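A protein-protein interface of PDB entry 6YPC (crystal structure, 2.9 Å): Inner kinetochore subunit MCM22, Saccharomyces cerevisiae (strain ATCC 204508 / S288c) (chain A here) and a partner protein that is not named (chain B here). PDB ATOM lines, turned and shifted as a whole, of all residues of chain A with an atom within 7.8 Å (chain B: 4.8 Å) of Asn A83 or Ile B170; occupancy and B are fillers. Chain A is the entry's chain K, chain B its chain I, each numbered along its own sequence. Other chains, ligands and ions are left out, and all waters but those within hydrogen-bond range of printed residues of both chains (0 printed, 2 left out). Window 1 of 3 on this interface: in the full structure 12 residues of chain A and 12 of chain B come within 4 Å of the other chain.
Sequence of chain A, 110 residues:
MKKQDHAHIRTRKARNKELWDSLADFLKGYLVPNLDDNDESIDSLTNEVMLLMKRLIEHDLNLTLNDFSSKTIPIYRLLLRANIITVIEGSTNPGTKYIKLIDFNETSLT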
ATOM      1  N   ARG A  77     -19.218  12.665 -18.462  1.00  0.00           N
ATOM      2  CA  ARG A  77     -18.242  11.826 -17.772  1.00  0.00           C
ATOM      3  C   ARG A  77     -17.855  10.613 -18.599  1.00  0.00           C
ATOM      4  O   ARG A  77     -16.721  10.125 -18.495  1.00  0.00           O
ATOM      5  CB  ARG A  77     -18.775  11.396 -16.413  1.00  0.00           C
ATOM      6  CG  ARG A  77     -18.454  12.431 -15.354  1.00  0.00           C
ATOM      7  CD  ARG A  77     -18.889  12.035 -13.952  1.00  0.00           C
ATOM      8  NE  ARG A  77     -20.329  11.829 -13.888  1.00  0.00           N
ATOM      9  CZ  ARG A  77     -21.164  12.647 -13.265  1.00  0.00           C
ATOM     10  NH1 ARG A  77     -20.705  13.737 -12.645  1.00  0.00           N
ATOM     11  NH2 ARG A  77     -22.461  12.369 -13.265  1.00  0.00           N
ATOM     12  N   LEU A  78     -18.775  10.122 -19.425  1.00  0.00           N
ATOM     13  CA  LEU A  78     -18.495   8.957 -20.250  1.00  0.00           C
ATOM     14  C   LEU A  78     -17.502   9.312 -21.345  1.00  0.00           C
ATOM     15  O   LEU A  78     -16.532   8.578 -21.588  1.00  0.00           O
ATOM     16  CB  LEU A  78     -19.800   8.433 -20.841  1.00  0.00           C
ATOM     17  CG  LEU A  78     -19.695   7.565 -22.081  1.00  0.00           C
ATOM     18  CD1 LEU A  78     -19.250   6.194 -21.662  1.00  0.00           C
ATOM     19  CD2 LEU A  78     -21.039   7.500 -22.800  1.00  0.00           C
ATOM     20  N   LEU A  79     -17.728  10.448 -22.011  1.00  0.00           N
ATOM     21  CA  LEU A  79     -16.765  10.947 -22.986  1.00  0.00           C
ATOM     22  C   LEU A  79     -15.411  11.160 -22.336  1.00  0.00           C
ATOM     23  O   LEU A  79     -14.375  10.758 -22.880  1.00  0.00           O
ATOM     24  CB  LEU A  79     -17.273  12.246 -23.604  1.00  0.00           C
ATOM     25  CG  LEU A  79     -18.699  12.109 -24.138  1.00  0.00           C
ATOM     26  CD1 LEU A  79     -19.385  13.465 -24.264  1.00  0.00           C
ATOM     27  CD2 LEU A  79     -18.652  11.384 -25.453  1.00  0.00           C
ATOM     28  N   LEU A  80     -15.403  11.757 -21.154  1.00  0.00           N
ATOM     29  CA  LEU A  80     -14.153  11.961 -20.444  1.00  0.00           C
ATOM     30  C   LEU A  80     -13.412  10.637 -20.248  1.00  0.00           C
ATOM     31  O   LEU A  80     -12.221  10.530 -20.561  1.00  0.00           O
ATOM     32  CB  LEU A  80     -14.445  12.649 -19.113  1.00  0.00           C
ATOM     33  CG  LEU A  80     -13.213  13.153 -18.375  1.00  0.00           C
ATOM     34  CD1 LEU A  80     -12.580  14.222 -19.199  1.00  0.00           C
ATOM     35  CD2 LEU A  80     -13.579  13.675 -17.013  1.00  0.00           C
ATOM     36  N   ARG A  81     -14.109   9.607 -19.754  1.00  0.00           N
ATOM     37  CA  ARG A  81     -13.444   8.339 -19.464  1.00  0.00           C
ATOM     38  C   ARG A  81     -12.823   7.746 -20.716  1.00  0.00           C
ATOM     39  O   ARG A  81     -11.658   7.316 -20.702  1.00  0.00           O
ATOM     40  CB  ARG A  81     -14.430   7.344 -18.852  1.00  0.00           C
ATOM     41  CG  ARG A  81     -14.333   7.247 -17.349  1.00  0.00           C
ATOM     42  CD  ARG A  81     -15.274   6.223 -16.803  1.00  0.00           C
ATOM     43  NE  ARG A  81     -16.633   6.539 -17.196  1.00  0.00           N
ATOM     44  CZ  ARG A  81     -17.375   5.760 -17.972  1.00  0.00           C
ATOM     45  NH1 ARG A  81     -16.874   4.609 -18.421  1.00  0.00           N
ATOM     46  NH2 ARG A  81     -18.612   6.137 -18.296  1.00  0.00           N
ATOM     47  N   ALA A  82     -13.596   7.729 -21.813  1.00  0.00           N
ATOM     48  CA  ALA A  82     -13.172   7.215 -23.114  1.00  0.00           C
ATOM     49  C   ALA A  82     -12.033   8.013 -23.735  1.00  0.00           C
ATOM     50  O   ALA A  82     -11.462   7.563 -24.735  1.00  0.00           O
ATOM     51  CB  ALA A  82     -14.360   7.195 -24.081  1.00  0.00           C
ATOM     52  N   ASN A  83     -11.701   9.178 -23.184  1.00  0.00           N
ATOM     53  CA  ASN A  83     -10.566   9.951 -23.660  1.00  0.00           C
ATOM     54  C   ASN A  83     -10.782  10.407 -25.088  1.00  0.00           C
ATOM     55  O   ASN A  83      -9.865  10.335 -25.899  1.00  0.00           O
ATOM     56  CB  ASN A  83      -9.264   9.152 -23.577  1.00  0.00           C
ATOM     57  CG  ASN A  83      -8.787   8.973 -22.169  1.00  0.00           C
ATOM     58  OD1 ASN A  83      -8.834   9.912 -21.362  1.00  0.00           O
ATOM     59  ND2 ASN A  83      -8.292   7.776 -21.858  1.00  0.00           N
ATOM     60  N   ILE A  84     -11.997  10.843 -25.411  1.00  0.00           N
ATOM     61  CA  ILE A  84     -12.299  11.237 -26.780  1.00  0.00           C
ATOM     62  C   ILE A  84     -12.824  12.665 -26.858  1.00  0.00           C
ATOM     63  O   ILE A  84     -13.423  13.051 -27.855  1.00  0.00           O
ATOM     64  CB  ILE A  84     -13.275  10.253 -27.450  1.00  0.00           C
ATOM     65  CG1 ILE A  84     -14.685  10.399 -26.882  1.00  0.00           C
ATOM     66  CG2 ILE A  84     -12.799   8.845 -27.286  1.00  0.00           C
ATOM     67  CD1 ILE A  84     -15.775  10.077 -27.909  1.00  0.00           C
ATOM     68  N   ILE A  85     -12.603  13.455 -25.812  1.00  0.00           N
ATOM     69  CA  ILE A  85     -12.903  14.880 -25.832  1.00  0.00           C
ATOM     70  C   ILE A  85     -11.762  15.633 -25.168  1.00  0.00           C
ATOM     71  O   ILE A  85     -11.032  15.093 -24.329  1.00  0.00           O
ATOM     72  CB  ILE A  85     -14.223  15.220 -25.120  1.00  0.00           C
ATOM     73  CG1 ILE A  85     -14.230  14.645 -23.712  1.00  0.00           C
ATOM     74  CG2 ILE A  85     -15.409  14.740 -25.917  1.00  0.00           C
ATOM     75  CD1 ILE A  85     -15.295  15.274 -22.856  1.00  0.00           C
ATOM     76  N   THR A  86     -11.618  16.895 -25.547  1.00  0.00           N
ATOM     77  CA  THR A  86     -10.667  17.812 -24.932  1.00  0.00           C
ATOM     78  C   THR A  86     -11.456  18.899 -24.224  1.00  0.00           C
ATOM     79  O   THR A  86     -12.409  19.448 -24.793  1.00  0.00           O
ATOM     80  CB  THR A  86      -9.728  18.411 -25.986  1.00  0.00           C
ATOM     81  OG1 THR A  86     -10.494  19.201 -26.908  1.00  0.00           O
ATOM     82  CG2 THR A  86      -8.983  17.319 -26.735  1.00  0.00           C
ATOM     83  N   LEU A 101     -14.706  17.214 -29.625  1.00  0.00           N
ATOM     84  CA  LEU A 101     -14.224  15.883 -29.927  1.00  0.00           C
ATOM     85  C   LEU A 101     -12.793  15.949 -30.428  1.00  0.00           C
ATOM     86  O   LEU A 101     -12.404  16.888 -31.127  1.00  0.00           O
ATOM     87  CB  LEU A 101     -15.096  15.230 -30.993  1.00  0.00           C
ATOM     88  CG  LEU A 101     -16.370  14.549 -30.536  1.00  0.00           C
ATOM     89  CD1 LEU A 101     -17.102  14.011 -31.749  1.00  0.00           C
ATOM     90  CD2 LEU A 101     -15.998  13.451 -29.586  1.00  0.00           C
ATOM     91  N   ILE A 102     -12.006  14.929 -30.088  1.00  0.00           N
ATOM     92  CA  ILE A 102     -10.690  14.783 -30.692  1.00  0.00           C
ATOM     93  C   ILE A 102     -10.910  14.652 -32.196  1.00  0.00           C
ATOM     94  O   ILE A 102     -12.042  14.416 -32.645  1.00  0.00           O
ATOM     95  CB  ILE A 102      -9.934  13.575 -30.122  1.00  0.00           C
ATOM     96  CG1 ILE A 102     -10.762  12.317 -30.324  1.00  0.00           C
ATOM     97  CG2 ILE A 102      -9.635  13.754 -28.639  1.00  0.00           C
ATOM     98  CD1 ILE A 102     -10.048  11.062 -29.920  1.00  0.00           C
ATOM     99  N   PHE A 104     -10.760  12.732 -35.517  1.00  0.00           N
ATOM    100  CA  PHE A 104     -10.576  11.387 -36.043  1.00  0.00           C
ATOM    101  C   PHE A 104     -10.158  11.377 -37.498  1.00  0.00           C
ATOM    102  O   PHE A 104      -9.623  10.363 -37.961  1.00  0.00           O
ATOM    103  CB  PHE A 104     -11.852  10.555 -35.895  1.00  0.00           C
ATOM    104  CG  PHE A 104     -12.268  10.358 -34.477  1.00  0.00           C
ATOM    105  CD1 PHE A 104     -11.575   9.489 -33.660  1.00  0.00           C
ATOM    106  CD2 PHE A 104     -13.334  11.057 -33.953  1.00  0.00           C
ATOM    107  CE1 PHE A 104     -11.940   9.318 -32.346  1.00  0.00           C
ATOM    108  CE2 PHE A 104     -13.702  10.885 -32.636  1.00  0.00           C
ATOM    109  CZ  PHE A 104     -13.004  10.012 -31.834  1.00  0.00           C
ATOM    110  N   LEU B 137      -7.786  -0.769 -29.646  1.00  0.00           N
ATOM    111  CA  LEU B 137      -7.042   0.329 -29.066  1.00  0.00           C
ATOM    112  C   LEU B 137      -7.766   0.870 -27.844  1.00  0.00           C
ATOM    113  O   LEU B 137      -7.137   1.151 -26.812  1.00  0.00           O
ATOM    114  CB  LEU B 137      -6.826   1.428 -30.095  1.00  0.00           C
ATOM    115  CG  LEU B 137      -5.959   2.494 -29.444  1.00  0.00           C
ATOM    116  CD1 LEU B 137      -4.566   1.932 -29.146  1.00  0.00           C
ATOM    117  CD2 LEU B 137      -5.920   3.721 -30.316  1.00  0.00           C
ATOM    118  N   TRP B 140      -7.389  -1.638 -25.197  1.00  0.00           N
ATOM    119  CA  TRP B 140      -6.019  -1.601 -24.715  1.00  0.00           C
ATOM    120  C   TRP B 140      -5.885  -0.792 -23.430  1.00  0.00           C
ATOM    121  O   TRP B 140      -5.062  -1.123 -22.573  1.00  0.00           O
ATOM    122  CB  TRP B 140      -5.134  -1.032 -25.813  1.00  0.00           C
ATOM    123  CG  TRP B 140      -3.742  -0.891 -25.401  1.00  0.00           C
ATOM    124  CD1 TRP B 140      -2.835  -1.890 -25.225  1.00  0.00           C
ATOM    125  CD2 TRP B 140      -3.070   0.328 -25.096  1.00  0.00           C
ATOM    126  NE1 TRP B 140      -1.631  -1.370 -24.829  1.00  0.00           N
ATOM    127  CE2 TRP B 140      -1.747  -0.007 -24.738  1.00  0.00           C
ATOM    128  CE3 TRP B 140      -3.456   1.674 -25.093  1.00  0.00           C
ATOM    129  CZ2 TRP B 140      -0.799   0.958 -24.386  1.00  0.00           C
ATOM    130  CZ3 TRP B 140      -2.511   2.637 -24.743  1.00  0.00           C
ATOM    131  CH2 TRP B 140      -1.200   2.270 -24.395  1.00  0.00           C
ATOM    132  N   GLN B 141      -6.718   0.237 -23.258  1.00  0.00           N
ATOM    133  CA  GLN B 141      -6.611   1.116 -22.098  1.00  0.00           C
ATOM    134  C   GLN B 141      -6.974   0.437 -20.777  1.00  0.00           C
ATOM    135  O   GLN B 141      -6.605   0.950 -19.718  1.00  0.00           O
ATOM    136  CB  GLN B 141      -7.491   2.352 -22.298  1.00  0.00           C
ATOM    137  CG  GLN B 141      -7.007   3.278 -23.389  1.00  0.00           C
ATOM    138  CD  GLN B 141      -8.043   4.336 -23.754  1.00  0.00           C
ATOM    139  OE1 GLN B 141      -7.784   5.545 -23.626  1.00  0.00           O
ATOM    140  NE2 GLN B 141      -9.231   3.891 -24.211  1.00  0.00           N
ATOM    141  N   TRP B 166      -4.941  10.601 -33.648  1.00  0.00           N
ATOM    142  CA  TRP B 166      -5.749  10.437 -32.452  1.00  0.00           C
ATOM    143  C   TRP B 166      -5.416   9.149 -31.735  1.00  0.00           C
ATOM    144  O   TRP B 166      -5.403   9.120 -30.502  1.00  0.00           O
ATOM    145  CB  TRP B 166      -7.223  10.498 -32.789  1.00  0.00           C
ATOM    146  CG  TRP B 166      -7.736   9.339 -33.527  1.00  0.00           C
ATOM    147  CD1 TRP B 166      -7.838   9.213 -34.880  1.00  0.00           C
ATOM    148  CD2 TRP B 166      -8.287   8.144 -32.967  1.00  0.00           C
ATOM    149  NE1 TRP B 166      -8.407   8.000 -35.197  1.00  0.00           N
ATOM    150  CE2 TRP B 166      -8.691   7.327 -34.041  1.00  0.00           C
ATOM    151  CE3 TRP B 166      -8.478   7.687 -31.664  1.00  0.00           C
ATOM    152  CZ2 TRP B 166      -9.267   6.073 -33.853  1.00  0.00           C
ATOM    153  CZ3 TRP B 166      -9.062   6.435 -31.476  1.00  0.00           C
ATOM    154  CH2 TRP B 166      -9.442   5.643 -32.565  1.00  0.00           C
ATOM    155  N   LYS B 167      -5.096   8.091 -32.473  1.00  0.00           N
ATOM    156  CA  LYS B 167      -4.572   6.915 -31.798  1.00  0.00           C
ATOM    157  C   LYS B 167      -3.300   7.229 -31.009  1.00  0.00           C
ATOM    158  O   LYS B 167      -3.013   6.544 -30.022  1.00  0.00           O
ATOM    159  CB  LYS B 167      -4.322   5.790 -32.808  1.00  0.00           C
ATOM    160  CG  LYS B 167      -5.526   5.461 -33.706  1.00  0.00           C
ATOM    161  CD  LYS B 167      -5.353   4.096 -34.363  1.00  0.00           C
ATOM    162  CE  LYS B 167      -6.566   3.693 -35.189  1.00  0.00           C
ATOM    163  NZ  LYS B 167      -6.462   2.285 -35.719  1.00  0.00           N
ATOM    164  N   LEU B 168      -2.555   8.276 -31.378  1.00  0.00           N
ATOM    165  CA  LEU B 168      -1.253   8.485 -30.746  1.00  0.00           C
ATOM    166  C   LEU B 168      -1.380   9.039 -29.340  1.00  0.00           C
ATOM    167  O   LEU B 168      -0.685   8.588 -28.415  1.00  0.00           O
ATOM    168  CB  LEU B 168      -0.392   9.415 -31.591  1.00  0.00           C
ATOM    169  CG  LEU B 168      -0.008   8.706 -32.884  1.00  0.00           C
ATOM    170  CD1 LEU B 168       0.296   9.707 -33.981  1.00  0.00           C
ATOM    171  CD2 LEU B 168       1.156   7.729 -32.618  1.00  0.00           C
ATOM    172  N   SER B 169      -2.241  10.029 -29.167  1.00  0.00           N
ATOM    173  CA  SER B 169      -2.390  10.606 -27.843  1.00  0.00           C
ATOM    174  C   SER B 169      -3.016   9.603 -26.889  1.00  0.00           C
ATOM    175  O   SER B 169      -2.572   9.469 -25.743  1.00  0.00           O
ATOM    176  CB  SER B 169      -3.219  11.873 -27.934  1.00  0.00           C
ATOM    177  OG  SER B 169      -4.323  11.617 -28.770  1.00  0.00           O
ATOM    178  N   ILE B 170      -4.037   8.878 -27.347  1.00  0.00           N
ATOM    179  CA  ILE B 170      -4.605   7.772 -26.584  1.00  0.00           C
ATOM    180  C   ILE B 170      -3.454   6.959 -26.007  1.00  0.00           C
ATOM    181  O   ILE B 170      -3.392   6.707 -24.792  1.00  0.00           O
ATOM    182  CB  ILE B 170      -5.507   6.890 -27.465  1.00  0.00           C
ATOM    183  CG1 ILE B 170      -6.774   7.632 -27.865  1.00  0.00           C
ATOM    184  CG2 ILE B 170      -5.870   5.617 -26.744  1.00  0.00           C
ATOM    185  CD1 ILE B 170      -7.953   7.370 -26.967  1.00  0.00           C
ATOM    186  N   ILE B 171      -2.524   6.577 -26.883  1.00  0.00           N
ATOM    187  CA  ILE B 171      -1.334   5.864 -26.450  1.00  0.00           C
ATOM    188  C   ILE B 171      -0.472   6.734 -25.539  1.00  0.00           C
ATOM    189  O   ILE B 171       0.018   6.264 -24.498  1.00  0.00           O
ATOM    190  CB  ILE B 171      -0.551   5.355 -27.677  1.00  0.00           C
ATOM    191  CG1 ILE B 171      -1.409   4.401 -28.504  1.00  0.00           C
ATOM    192  CG2 ILE B 171       0.750   4.682 -27.275  1.00  0.00           C
ATOM    193  CD1 ILE B 171      -0.874   4.166 -29.909  1.00  0.00           C
ATOM    194  N   LYS B 172      -0.261   8.008 -25.895  1.00  0.00           N
ATOM    195  CA  LYS B 172       0.712   8.756 -25.110  1.00  0.00           C
ATOM    196  C   LYS B 172       0.135   9.109 -23.744  1.00  0.00           C
ATOM    197  O   LYS B 172       0.817   8.994 -22.721  1.00  0.00           O
ATOM    198  CB  LYS B 172       1.201  10.013 -25.837  1.00  0.00           C
ATOM    199  CG  LYS B 172       2.224  10.792 -24.936  1.00  0.00           C
ATOM    200  CD  LYS B 172       2.760  12.126 -25.481  1.00  0.00           C
ATOM    201  CE  LYS B 172       1.705  12.869 -26.308  1.00  0.00           C
ATOM    202  NZ  LYS B 172       1.999  14.329 -26.588  1.00  0.00           N
ATOM    203  N   ARG B 173      -1.134   9.525 -23.708  1.00  0.00           N
ATOM    204  CA  ARG B 173      -1.845   9.712 -22.450  1.00  0.00           C
ATOM    205  C   ARG B 173      -1.648   8.518 -21.537  1.00  0.00           C
ATOM    206  O   ARG B 173      -1.318   8.669 -20.360  1.00  0.00           O
ATOM    207  CB  ARG B 173      -3.342   9.924 -22.712  1.00  0.00           C
ATOM    208  CG  ARG B 173      -4.156   9.412 -21.553  1.00  0.00           C
ATOM    209  CD  ARG B 173      -5.604   9.756 -21.630  1.00  0.00           C
ATOM    210  NE  ARG B 173      -6.147   9.663 -20.281  1.00  0.00           N
ATOM    211  CZ  ARG B 173      -6.210  10.687 -19.429  1.00  0.00           C
ATOM    212  NH1 ARG B 173      -5.799  11.885 -19.809  1.00  0.00           N
ATOM    213  NH2 ARG B 173      -6.693  10.524 -18.200  1.00  0.00           N
ATOM    214  N   CYS B 174      -1.820   7.317 -22.080  1.00  0.00           N
ATOM    215  CA  CYS B 174      -1.833   6.129 -21.243  1.00  0.00           C
ATOM    216  C   CYS B 174      -0.439   5.763 -20.760  1.00  0.00           C
ATOM    217  O   CYS B 174      -0.279   5.279 -19.636  1.00  0.00           O
ATOM    218  CB  CYS B 174      -2.459   4.977 -22.008  1.00  0.00           C
ATOM    219  SG  CYS B 174      -2.971   3.671 -20.914  1.00  0.00           S
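The guanidinium group (NE) of Arg B173 sits at hydrogen-bond distance from the side-chain amide oxygen (OD1) of Asn A83 (2.9 Å). The side-chain amide nitrogen (ND2) of Asn A83 sits at hydrogen-bond distance from the side-chain amide oxygen (OE1) of Gln B141 (2.9 Å).
O of Trp B166 lies within hydrogen-bond range of OG of Ser B169.
Among the printed residues, merely in contact across the chains: Phe A104 with Trp B166 and Asn A83 with Ile B170.
Arg A77 touches none of the printed residues of chain B. Asn A83 touches three residues of chain B. Ile A102 touches none of the printed residues of chain B. Printed residues of chain B within 4 Å of Phe A104: Trp B166 (3.6 Å). Printed residues of chain A within 4 Å of Gln B141: Asn A83. Of the printed residues of chain A, Trp B166 touches Phe A104. No residue of chain A comes within 4 Å of Ser B169. Ile B170 touches one residue of chain A. Of the printed residues of chain A, Arg B173 touches Asn A83 (2.9 Å).
Hydrophobic or aromatic side chains of chain A within 4 Å of the printed part of chain B: Phe A104. Of the 12 printed residues of chain B, 4 touch a printed residue of chain A. Printed residues of chain B that touch a printed residue of chain A: Gln B141, Trp B166, Ile B170 and Arg B173. Among the printed residues, 4 pairs touch across the chains. Among the printed residues, no Asp or Glu carboxylate lies within 4 Å of a Lys or Arg side-chain nitrogen of the other chain.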
